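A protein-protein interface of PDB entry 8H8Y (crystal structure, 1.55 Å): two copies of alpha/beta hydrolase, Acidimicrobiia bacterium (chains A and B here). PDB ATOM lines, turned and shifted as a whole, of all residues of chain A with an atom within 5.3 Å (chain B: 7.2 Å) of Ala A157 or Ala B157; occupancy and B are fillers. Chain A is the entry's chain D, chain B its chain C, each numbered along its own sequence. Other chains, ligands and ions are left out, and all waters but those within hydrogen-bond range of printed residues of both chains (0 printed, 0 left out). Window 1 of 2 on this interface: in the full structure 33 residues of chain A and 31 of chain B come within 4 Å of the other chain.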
ATOM      1  N   VAL A 111      28.414   2.565 -37.055  1.00  0.00           N
ATOM      2  CA  VAL A 111      27.321   1.570 -36.977  1.00  0.00           C
ATOM      3  C   VAL A 111      27.081   0.928 -38.335  1.00  0.00           C
ATOM      4  O   VAL A 111      26.891  -0.283 -38.375  1.00  0.00           O
ATOM      5  CB  VAL A 111      26.030   2.169 -36.393  1.00  0.00           C
ATOM      6  CG1 VAL A 111      25.015   1.074 -36.063  1.00  0.00           C
ATOM      7  CG2 VAL A 111      26.322   3.002 -35.151  1.00  0.00           C
ATOM      8  N   SER A 153      27.697   7.686 -28.071  1.00  0.00           N
ATOM      9  CA  SER A 153      26.300   7.196 -28.291  1.00  0.00           C
ATOM     10  C   SER A 153      26.267   6.169 -29.423  1.00  0.00           C
ATOM     11  O   SER A 153      25.742   5.080 -29.228  1.00  0.00           O
ATOM     12  CB  SER A 153      25.370   8.322 -28.556  1.00  0.00           C
ATOM     13  OG  SER A 153      25.538   9.279 -27.502  1.00  0.00           O
ATOM     14  N   VAL A 154      26.857   6.467 -30.580  1.00  0.00           N
ATOM     15  CA  VAL A 154      26.740   5.537 -31.738  1.00  0.00           C
ATOM     16  C   VAL A 154      27.619   4.297 -31.472  1.00  0.00           C
ATOM     17  O   VAL A 154      27.285   3.195 -31.909  1.00  0.00           O
ATOM     18  CB  VAL A 154      27.073   6.233 -33.074  1.00  0.00           C
ATOM     19  CG1 VAL A 154      26.044   7.303 -33.396  1.00  0.00           C
ATOM     20  CG2 VAL A 154      28.489   6.818 -33.101  1.00  0.00           C
ATOM     21  N   ARG A 155      28.734   4.434 -30.761  1.00  0.00           N
ATOM     22  CA  ARG A 155      29.536   3.243 -30.435  1.00  0.00           C
ATOM     23  C   ARG A 155      28.737   2.315 -29.532  1.00  0.00           C
ATOM     24  O   ARG A 155      28.889   1.099 -29.675  1.00  0.00           O
ATOM     25  CB  ARG A 155      30.861   3.626 -29.774  1.00  0.00           C
ATOM     26  CG  ARG A 155      31.825   4.370 -30.690  1.00  0.00           C
ATOM     27  CD  ARG A 155      32.377   3.465 -31.782  1.00  0.00           C
ATOM     28  NE  ARG A 155      33.579   4.053 -32.368  1.00  0.00           N
ATOM     29  CZ  ARG A 155      34.255   3.556 -33.410  1.00  0.00           C
ATOM     30  NH1 ARG A 155      33.861   2.472 -34.051  1.00  0.00           N
ATOM     31  NH2 ARG A 155      35.363   4.154 -33.809  1.00  0.00           N
ATOM     32  N   ALA A 156      27.849   2.856 -28.700  1.00  0.00           N
ATOM     33  CA  ALA A 156      27.004   1.997 -27.841  1.00  0.00           C
ATOM     34  C   ALA A 156      26.037   1.181 -28.716  1.00  0.00           C
ATOM     35  O   ALA A 156      25.777   0.021 -28.360  1.00  0.00           O
ATOM     36  CB  ALA A 156      26.235   2.828 -26.866  1.00  0.00           C
ATOM     37  N   ALA A 157      25.520   1.768 -29.786  1.00  0.00           N
ATOM     38  CA  ALA A 157      24.658   1.037 -30.739  1.00  0.00           C
ATOM     39  C   ALA A 157      25.443  -0.127 -31.349  1.00  0.00           C
ATOM     40  O   ALA A 157      24.859  -1.226 -31.479  1.00  0.00           O
ATOM     41  CB  ALA A 157      24.113   1.963 -31.787  1.00  0.00           C
ATOM     42  N   ALA A 158      26.675   0.117 -31.810  1.00  0.00           N
ATOM     43  CA  ALA A 158      27.492  -0.915 -32.473  1.00  0.00           C
ATOM     44  C   ALA A 158      27.676  -2.075 -31.504  1.00  0.00           C
ATOM     45  O   ALA A 158      27.494  -3.247 -31.896  1.00  0.00           O
ATOM     46  CB  ALA A 158      28.839  -0.403 -32.916  1.00  0.00           C
ATOM     47  N   THR A 159      28.064  -1.776 -30.274  1.00  0.00           N
ATOM     48  CA  THR A 159      28.280  -2.835 -29.271  1.00  0.00           C
ATOM     49  C   THR A 159      26.981  -3.604 -29.007  1.00  0.00           C
ATOM     50  O   THR A 159      27.015  -4.841 -28.946  1.00  0.00           O
ATOM     51  CB  THR A 159      28.913  -2.267 -28.011  1.00  0.00           C
ATOM     52  OG1 THR A 159      30.165  -1.709 -28.375  1.00  0.00           O
ATOM     53  CG2 THR A 159      29.113  -3.335 -26.959  1.00  0.00           C
ATOM     54  N   MET A 160      25.849  -2.903 -28.879  1.00  0.00           N
ATOM     55  CA  MET A 160      24.568  -3.592 -28.634  1.00  0.00           C
ATOM     56  C   MET A 160      24.134  -4.373 -29.870  1.00  0.00           C
ATOM     57  O   MET A 160      23.574  -5.464 -29.734  1.00  0.00           O
ATOM     58  CB  MET A 160      23.476  -2.613 -28.205  1.00  0.00           C
ATOM     59  CG  MET A 160      22.146  -3.289 -27.863  1.00  0.00           C
ATOM     60  SD  MET A 160      22.282  -4.578 -26.579  1.00  0.00           S
ATOM     61  CE  MET A 160      22.672  -3.574 -25.150  1.00  0.00           C
ATOM     62  N   LEU A 161      24.472  -3.899 -31.069  1.00  0.00           N
ATOM     63  CA  LEU A 161      24.156  -4.711 -32.291  1.00  0.00           C
ATOM     64  C   LEU A 161      24.913  -6.037 -32.232  1.00  0.00           C
ATOM     65  O   LEU A 161      24.342  -7.085 -32.545  1.00  0.00           O
ATOM     66  CB  LEU A 161      24.529  -3.908 -33.549  1.00  0.00           C
ATOM     67  CG  LEU A 161      24.178  -4.579 -34.873  1.00  0.00           C
ATOM     68  CD1 LEU A 161      22.697  -4.872 -35.021  1.00  0.00           C
ATOM     69  CD2 LEU A 161      24.682  -3.709 -36.032  1.00  0.00           C
ATOM     70  N   VAL A 162      26.181  -5.986 -31.861  1.00  0.00           N
ATOM     71  CA  VAL A 162      27.001  -7.211 -31.715  1.00  0.00           C
ATOM     72  C   VAL A 162      26.328  -8.148 -30.714  1.00  0.00           C
ATOM     73  O   VAL A 162      26.204  -9.349 -31.007  1.00  0.00           O
ATOM     74  CB  VAL A 162      28.429  -6.859 -31.276  1.00  0.00           C
ATOM     75  CG1 VAL A 162      29.160  -8.110 -30.807  1.00  0.00           C
ATOM     76  CG2 VAL A 162      29.176  -6.128 -32.384  1.00  0.00           C
ATOM     77  N   LEU B 103      17.959  -0.278 -40.905  1.00  0.00           N
ATOM     78  CA  LEU B 103      18.828   0.260 -39.837  1.00  0.00           C
ATOM     79  C   LEU B 103      18.751   1.782 -39.840  1.00  0.00           C
ATOM     80  O   LEU B 103      18.617   2.367 -38.757  1.00  0.00           O
ATOM     81  CB  LEU B 103      20.260  -0.238 -40.036  1.00  0.00           C
ATOM     82  CG  LEU B 103      21.252   0.363 -39.050  1.00  0.00           C
ATOM     83  CD1 LEU B 103      20.983  -0.124 -37.628  1.00  0.00           C
ATOM     84  CD2 LEU B 103      22.671   0.056 -39.482  1.00  0.00           C
ATOM     85  N   PHE B 107      17.057   4.289 -36.820  1.00  0.00           N
ATOM     86  CA  PHE B 107      17.954   5.318 -36.240  1.00  0.00           C
ATOM     87  C   PHE B 107      17.238   6.677 -36.198  1.00  0.00           C
ATOM     88  O   PHE B 107      17.401   7.451 -35.241  1.00  0.00           O
ATOM     89  CB  PHE B 107      19.261   5.383 -37.043  1.00  0.00           C
ATOM     90  CG  PHE B 107      20.244   6.334 -36.422  1.00  0.00           C
ATOM     91  CD1 PHE B 107      20.492   7.577 -36.984  1.00  0.00           C
ATOM     92  CD2 PHE B 107      20.934   5.960 -35.286  1.00  0.00           C
ATOM     93  CE1 PHE B 107      21.386   8.445 -36.367  1.00  0.00           C
ATOM     94  CE2 PHE B 107      21.867   6.812 -34.717  1.00  0.00           C
ATOM     95  CZ  PHE B 107      22.076   8.041 -35.259  1.00  0.00           C
ATOM     96  N   CYS B 110      14.493   6.603 -33.456  1.00  0.00           N
ATOM     97  CA  CYS B 110      14.923   6.209 -32.087  1.00  0.00           C
ATOM     98  C   CYS B 110      16.082   7.068 -31.611  1.00  0.00           C
ATOM     99  O   CYS B 110      16.289   7.087 -30.395  1.00  0.00           O
ATOM    100  CB  CYS B 110      15.318   4.746 -31.989  1.00  0.00           C
ATOM    101  SG  CYS B 110      13.941   3.620 -32.308  1.00  0.00           S
ATOM    102  N   VAL B 111      16.833   7.708 -32.505  1.00  0.00           N
ATOM    103  CA  VAL B 111      18.007   8.509 -32.079  1.00  0.00           C
ATOM    104  C   VAL B 111      17.923   9.968 -32.571  1.00  0.00           C
ATOM    105  O   VAL B 111      18.262  10.878 -31.813  1.00  0.00           O
ATOM    106  CB  VAL B 111      19.333   7.832 -32.497  1.00  0.00           C
ATOM    107  CG1 VAL B 111      20.488   8.490 -31.765  1.00  0.00           C
ATOM    108  CG2 VAL B 111      19.325   6.332 -32.262  1.00  0.00           C
ATOM    109  N   PRO B 114      15.209  12.031 -30.244  1.00  0.00           N
ATOM    110  CA  PRO B 114      15.701  12.503 -28.959  1.00  0.00           C
ATOM    111  C   PRO B 114      16.915  13.441 -29.054  1.00  0.00           C
ATOM    112  O   PRO B 114      17.039  14.366 -28.196  1.00  0.00           O
ATOM    113  CB  PRO B 114      16.003  11.197 -28.187  1.00  0.00           C
ATOM    114  CG  PRO B 114      16.213  10.157 -29.256  1.00  0.00           C
ATOM    115  CD  PRO B 114      15.287  10.576 -30.389  1.00  0.00           C
ATOM    116  N   THR B 137      13.210   6.186 -23.984  1.00  0.00           N
ATOM    117  CA  THR B 137      13.863   5.406 -25.055  1.00  0.00           C
ATOM    118  C   THR B 137      13.110   4.073 -25.112  1.00  0.00           C
ATOM    119  O   THR B 137      11.942   4.078 -25.450  1.00  0.00           O
ATOM    120  CB  THR B 137      15.380   5.296 -24.798  1.00  0.00           C
ATOM    121  OG1 THR B 137      15.664   4.603 -23.569  1.00  0.00           O
ATOM    122  CG2 THR B 137      16.029   6.667 -24.717  1.00  0.00           C
ATOM    123  N   GLY B 141      16.701  -1.231 -25.474  1.00  0.00           N
ATOM    124  CA  GLY B 141      18.061  -0.659 -25.520  1.00  0.00           C
ATOM    125  C   GLY B 141      18.977  -1.239 -24.461  1.00  0.00           C
ATOM    126  O   GLY B 141      20.203  -1.092 -24.610  1.00  0.00           O
ATOM    127  N   PRO B 149      16.720  -6.932 -33.333  1.00  0.00           N
ATOM    128  CA  PRO B 149      18.120  -6.627 -33.073  1.00  0.00           C
ATOM    129  C   PRO B 149      18.486  -5.183 -33.455  1.00  0.00           C
ATOM    130  O   PRO B 149      19.292  -4.533 -32.754  1.00  0.00           O
ATOM    131  CB  PRO B 149      18.913  -7.628 -33.938  1.00  0.00           C
ATOM    132  CG  PRO B 149      17.915  -8.010 -35.028  1.00  0.00           C
ATOM    133  CD  PRO B 149      16.563  -8.003 -34.344  1.00  0.00           C
ATOM    134  N   LEU B 150      17.970  -4.698 -34.586  1.00  0.00           N
ATOM    135  CA  LEU B 150      18.338  -3.347 -35.070  1.00  0.00           C
ATOM    136  C   LEU B 150      17.713  -2.322 -34.135  1.00  0.00           C
ATOM    137  O   LEU B 150      18.374  -1.338 -33.761  1.00  0.00           O
ATOM    138  CB  LEU B 150      17.849  -3.159 -36.508  1.00  0.00           C
ATOM    139  CG  LEU B 150      18.760  -3.677 -37.616  1.00  0.00           C
ATOM    140  CD1 LEU B 150      19.111  -5.119 -37.436  1.00  0.00           C
ATOM    141  CD2 LEU B 150      18.130  -3.440 -38.972  1.00  0.00           C
ATOM    142  N   TYR B 151      16.440  -2.535 -33.801  1.00  0.00           N
ATOM    143  CA  TYR B 151      15.701  -1.656 -32.862  1.00  0.00           C
ATOM    144  C   TYR B 151      16.464  -1.558 -31.530  1.00  0.00           C
ATOM    145  O   TYR B 151      16.665  -0.434 -31.015  1.00  0.00           O
ATOM    146  CB  TYR B 151      14.304  -2.242 -32.681  1.00  0.00           C
ATOM    147  CG  TYR B 151      13.351  -1.474 -31.805  1.00  0.00           C
ATOM    148  CD1 TYR B 151      12.819  -0.253 -32.207  1.00  0.00           C
ATOM    149  CD2 TYR B 151      12.929  -2.027 -30.619  1.00  0.00           C
ATOM    150  CE1 TYR B 151      11.865   0.403 -31.443  1.00  0.00           C
ATOM    151  CE2 TYR B 151      11.994  -1.383 -29.837  1.00  0.00           C
ATOM    152  CZ  TYR B 151      11.485  -0.158 -30.238  1.00  0.00           C
ATOM    153  OH  TYR B 151      10.556   0.438 -29.412  1.00  0.00           O
ATOM    154  N   SER B 152      16.822  -2.707 -30.979  1.00  0.00           N
ATOM    155  CA  SER B 152      17.547  -2.774 -29.691  1.00  0.00           C
ATOM    156  C   SER B 152      18.817  -1.925 -29.817  1.00  0.00           C
ATOM    157  O   SER B 152      19.097  -1.114 -28.881  1.00  0.00           O
ATOM    158  CB  SER B 152      17.832  -4.183 -29.276  1.00  0.00           C
ATOM    159  OG  SER B 152      18.867  -4.231 -28.283  1.00  0.00           O
ATOM    160  N   SER B 153      19.595  -2.105 -30.895  1.00  0.00           N
ATOM    161  CA  SER B 153      20.889  -1.411 -31.073  1.00  0.00           C
ATOM    162  C   SER B 153      20.704   0.103 -31.053  1.00  0.00           C
ATOM    163  O   SER B 153      21.444   0.770 -30.341  1.00  0.00           O
ATOM    164  CB  SER B 153      21.626  -1.865 -32.296  1.00  0.00           C
ATOM    165  OG  SER B 153      21.656  -3.287 -32.267  1.00  0.00           O
ATOM    166  N   VAL B 154      19.748   0.643 -31.813  1.00  0.00           N
ATOM    167  CA  VAL B 154      19.604   2.115 -31.890  1.00  0.00           C
ATOM    168  C   VAL B 154      19.022   2.661 -30.575  1.00  0.00           C
ATOM    169  O   VAL B 154      19.397   3.786 -30.182  1.00  0.00           O
ATOM    170  CB  VAL B 154      18.831   2.569 -33.136  1.00  0.00           C
ATOM    171  CG1 VAL B 154      19.615   2.209 -34.396  1.00  0.00           C
ATOM    172  CG2 VAL B 154      17.403   2.038 -33.198  1.00  0.00           C
ATOM    173  N   ARG B 155      18.138   1.925 -29.896  1.00  0.00           N
ATOM    174  CA  ARG B 155      17.636   2.334 -28.559  1.00  0.00           C
ATOM    175  C   ARG B 155      18.830   2.463 -27.602  1.00  0.00           C
ATOM    176  O   ARG B 155      18.827   3.438 -26.788  1.00  0.00           O
ATOM    177  CB  ARG B 155      16.591   1.368 -28.024  1.00  0.00           C
ATOM    178  CG  ARG B 155      15.287   1.432 -28.807  1.00  0.00           C
ATOM    179  CD  ARG B 155      14.561   2.756 -28.654  1.00  0.00           C
ATOM    180  NE  ARG B 155      13.191   2.620 -29.105  1.00  0.00           N
ATOM    181  CZ  ARG B 155      12.287   3.584 -29.142  1.00  0.00           C
ATOM    182  NH1 ARG B 155      12.589   4.844 -28.876  1.00  0.00           N
ATOM    183  NH2 ARG B 155      11.064   3.297 -29.569  1.00  0.00           N
ATOM    184  N   ALA B 156      19.841   1.589 -27.714  1.00  0.00           N
ATOM    185  CA  ALA B 156      21.028   1.670 -26.820  1.00  0.00           C
ATOM    186  C   ALA B 156      21.777   2.979 -27.083  1.00  0.00           C
ATOM    187  O   ALA B 156      22.329   3.585 -26.138  1.00  0.00           O
ATOM    188  CB  ALA B 156      21.921   0.471 -27.056  1.00  0.00           C
ATOM    189  N   ALA B 157      21.857   3.402 -28.342  1.00  0.00           N
ATOM    190  CA  ALA B 157      22.486   4.701 -28.674  1.00  0.00           C
ATOM    191  C   ALA B 157      21.738   5.833 -27.980  1.00  0.00           C
ATOM    192  O   ALA B 157      22.373   6.751 -27.463  1.00  0.00           O
ATOM    193  CB  ALA B 157      22.584   4.925 -30.168  1.00  0.00           C
ATOM    194  N   ALA B 158      20.405   5.828 -28.041  1.00  0.00           N
ATOM    195  CA  ALA B 158      19.610   6.918 -27.453  1.00  0.00           C
ATOM    196  C   ALA B 158      19.858   6.985 -25.946  1.00  0.00           C
ATOM    197  O   ALA B 158      20.121   8.075 -25.406  1.00  0.00           O
ATOM    198  CB  ALA B 158      18.163   6.733 -27.772  1.00  0.00           C
ATOM    199  N   THR B 159      19.853   5.858 -25.269  1.00  0.00           N
ATOM    200  CA  THR B 159      20.112   5.831 -23.821  1.00  0.00           C
ATOM    201  C   THR B 159      21.522   6.356 -23.543  1.00  0.00           C
ATOM    202  O   THR B 159      21.666   7.178 -22.606  1.00  0.00           O
ATOM    203  CB  THR B 159      19.872   4.440 -23.230  1.00  0.00           C
ATOM    204  OG1 THR B 159      18.501   4.139 -23.540  1.00  0.00           O
ATOM    205  CG2 THR B 159      20.152   4.407 -21.744  1.00  0.00           C
ATOM    206  N   MET B 160      22.518   5.936 -24.324  1.00  0.00           N
ATOM    207  CA  MET B 160      23.916   6.365 -24.060  1.00  0.00           C
ATOM    208  C   MET B 160      24.030   7.861 -24.373  1.00  0.00           C
ATOM    209  O   MET B 160      24.766   8.580 -23.661  1.00  0.00           O
ATOM    210  CB  MET B 160      24.944   5.547 -24.824  1.00  0.00           C
ATOM    211  CG  MET B 160      26.375   5.911 -24.504  1.00  0.00           C
ATOM    212  SD  MET B 160      26.805   5.875 -22.732  1.00  0.00           S
ATOM    213  CE  MET B 160      26.885   4.122 -22.402  1.00  0.00           C
ATOM    214  N   LEU B 161      23.272   8.360 -25.356  1.00  0.00           N
ATOM    215  CA  LEU B 161      23.306   9.807 -25.645  1.00  0.00           C
ATOM    216  C   LEU B 161      22.790  10.538 -24.404  1.00  0.00           C
ATOM    217  O   LEU B 161      23.399  11.536 -23.990  1.00  0.00           O
ATOM    218  CB  LEU B 161      22.470  10.106 -26.886  1.00  0.00           C
ATOM    219  CG  LEU B 161      22.437  11.573 -27.331  1.00  0.00           C
ATOM    220  CD1 LEU B 161      23.811  12.078 -27.681  1.00  0.00           C
ATOM    221  CD2 LEU B 161      21.477  11.776 -28.488  1.00  0.00           C
ATOM    222  N   VAL B 162      21.679  10.087 -23.848  1.00  0.00           N
ATOM    223  CA  VAL B 162      21.151  10.690 -22.594  1.00  0.00           C
ATOM    224  C   VAL B 162      22.237  10.735 -21.513  1.00  0.00           C
ATOM    225  O   VAL B 162      22.431  11.805 -20.877  1.00  0.00           O
ATOM    226  CB  VAL B 162      19.887   9.982 -22.097  1.00  0.00           C
ATOM    227  CG1 VAL B 162      19.488  10.458 -20.720  1.00  0.00           C
ATOM    228  CG2 VAL B 162      18.773  10.197 -23.106  1.00  0.00           C
ATOM    229  N   LYS B 163      22.920   9.635 -21.279  1.00  0.00           N
ATOM    230  CA  LYS B 163      23.958   9.578 -20.216  1.00  0.00           C
ATOM    231  C   LYS B 163      25.089  10.550 -20.531  1.00  0.00           C
ATOM    232  O   LYS B 163      25.558  11.230 -19.596  1.00  0.00           O
ATOM    233  CB  LYS B 163      24.474   8.161 -20.042  1.00  0.00           C
ATOM    234  CG  LYS B 163      23.399   7.196 -19.572  1.00  0.00           C
ATOM    235  CD  LYS B 163      23.959   5.836 -19.247  1.00  0.00           C
ATOM    236  CE  LYS B 163      22.939   4.916 -18.629  1.00  0.00           C
ATOM    237  NZ  LYS B 163      23.498   3.579 -18.351  1.00  0.00           N
ATOM    238  N   ASN B 164      25.426  10.724 -21.786  1.00  0.00           N
ATOM    239  CA  ASN B 164      26.490  11.657 -22.212  1.00  0.00           C
ATOM    240  C   ASN B 164      26.050  13.108 -22.001  1.00  0.00           C
ATOM    241  O   ASN B 164      26.852  13.882 -21.440  1.00  0.00           O
ATOM    242  CB  ASN B 164      26.881  11.405 -23.650  1.00  0.00           C
ATOM    243  CG  ASN B 164      28.014  10.429 -23.785  1.00  0.00           C
ATOM    244  OD1 ASN B 164      29.175  10.813 -23.667  1.00  0.00           O
ATOM    245  ND2 ASN B 164      27.666   9.175 -23.956  1.00  0.00           N
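The side-chain hydroxyl (OG) of Ser B153 sits close to the backbone NH (N) of Leu A161 (3.1 Å). N of Leu B161 lies close to OG of Ser A153.
The backbone carbonyl oxygen (O) of Pro B149 is in hydrogen-bond range of the side-chain hydroxyl (OG) of Ser B153 (2.7 Å). The backbone carbonyl oxygen of Met B160 sits at hydrogen-bond distance from the side-chain amide nitrogen of Asn B164, at 3.0 Å.
O of Ser A153 touches CB of Ala B157, at 3.3 Å. OG of Ser A153 touches C of Met B160, 3.8 Å away. Ala A156 touches Met B160 (CB to CB, 3.6 Å). O of Ser B153 touches CA of Ala A157, at 3.2 Å. Ala A157 touches Ala B157. Gly B141 touches Met A160. Met A160 touches Ser B152. OG of Ser B153 touches C of Met A160, 3.6 Å away. Met A160 touches Ala B156 (CB to CB, 3.6 Å).
Of the printed residues of chain B, Ala A156 touches Met B160 (3.6 Å). Ala A157 touches just these residues of chain B: Ser B153 (3.2 Å) and Ala B157 (3.7 Å). Printed residues of chain B within 4 Å of Leu A161: Ser B153 (2.9 Å). Of the printed residues of chain A, Ser B152 touches Met A160. Val B154 touches none of the printed residues of chain A. Printed residues of chain A within 4 Å of Ala B156: Met A160. Ala B157 touches just these residues of chain A: Ser A153 and Ala A157. Printed residues of chain A within 4 Å of Leu B161: Ser A153 (3.0 Å). The nearest residue of chain B that does not touch Ala A157 is Val B154 (4.5 Å). The nearest printed residue of chain B that does not touch Leu A161 is Pro B149 (4.1 Å).
Printed residues of chain B that touch a printed residue of chain A: Gly B141, Ser B152, Ser B153, Ala B156, Ala B157, Met B160 and Leu B161. Printed residues of chain A that touch a printed residue of chain B: Ser A153, Ala A156, Ala A157, Met A160 and Leu A161. Hydrophobic or aromatic side chains of chain A that line the printed part of chain B: Ala A156, Ala A157, Met A160 and Leu A161. Among the printed residues, 11 pairs touch across the chains. Among the printed residues, no Asp or Glu carboxylate lies within 4 Å of a Lys or Arg side-chain nitrogen of the other chain.
Ser A153 touches Met B160, and with the chains exchanged Met A160 touches Ser B153. Ser A153 touches Leu B161, and with the chains exchanged Leu A161 touches Ser B153. Ala A156 touches Met B160, and with the chains exchanged Met A160 touches Ala B156. Ala A157 touches its own counterpart, Ala B157. Of the 11 pairs that touch across the chains among the printed residues, 9 have their exchanged pair printed and touching as well.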
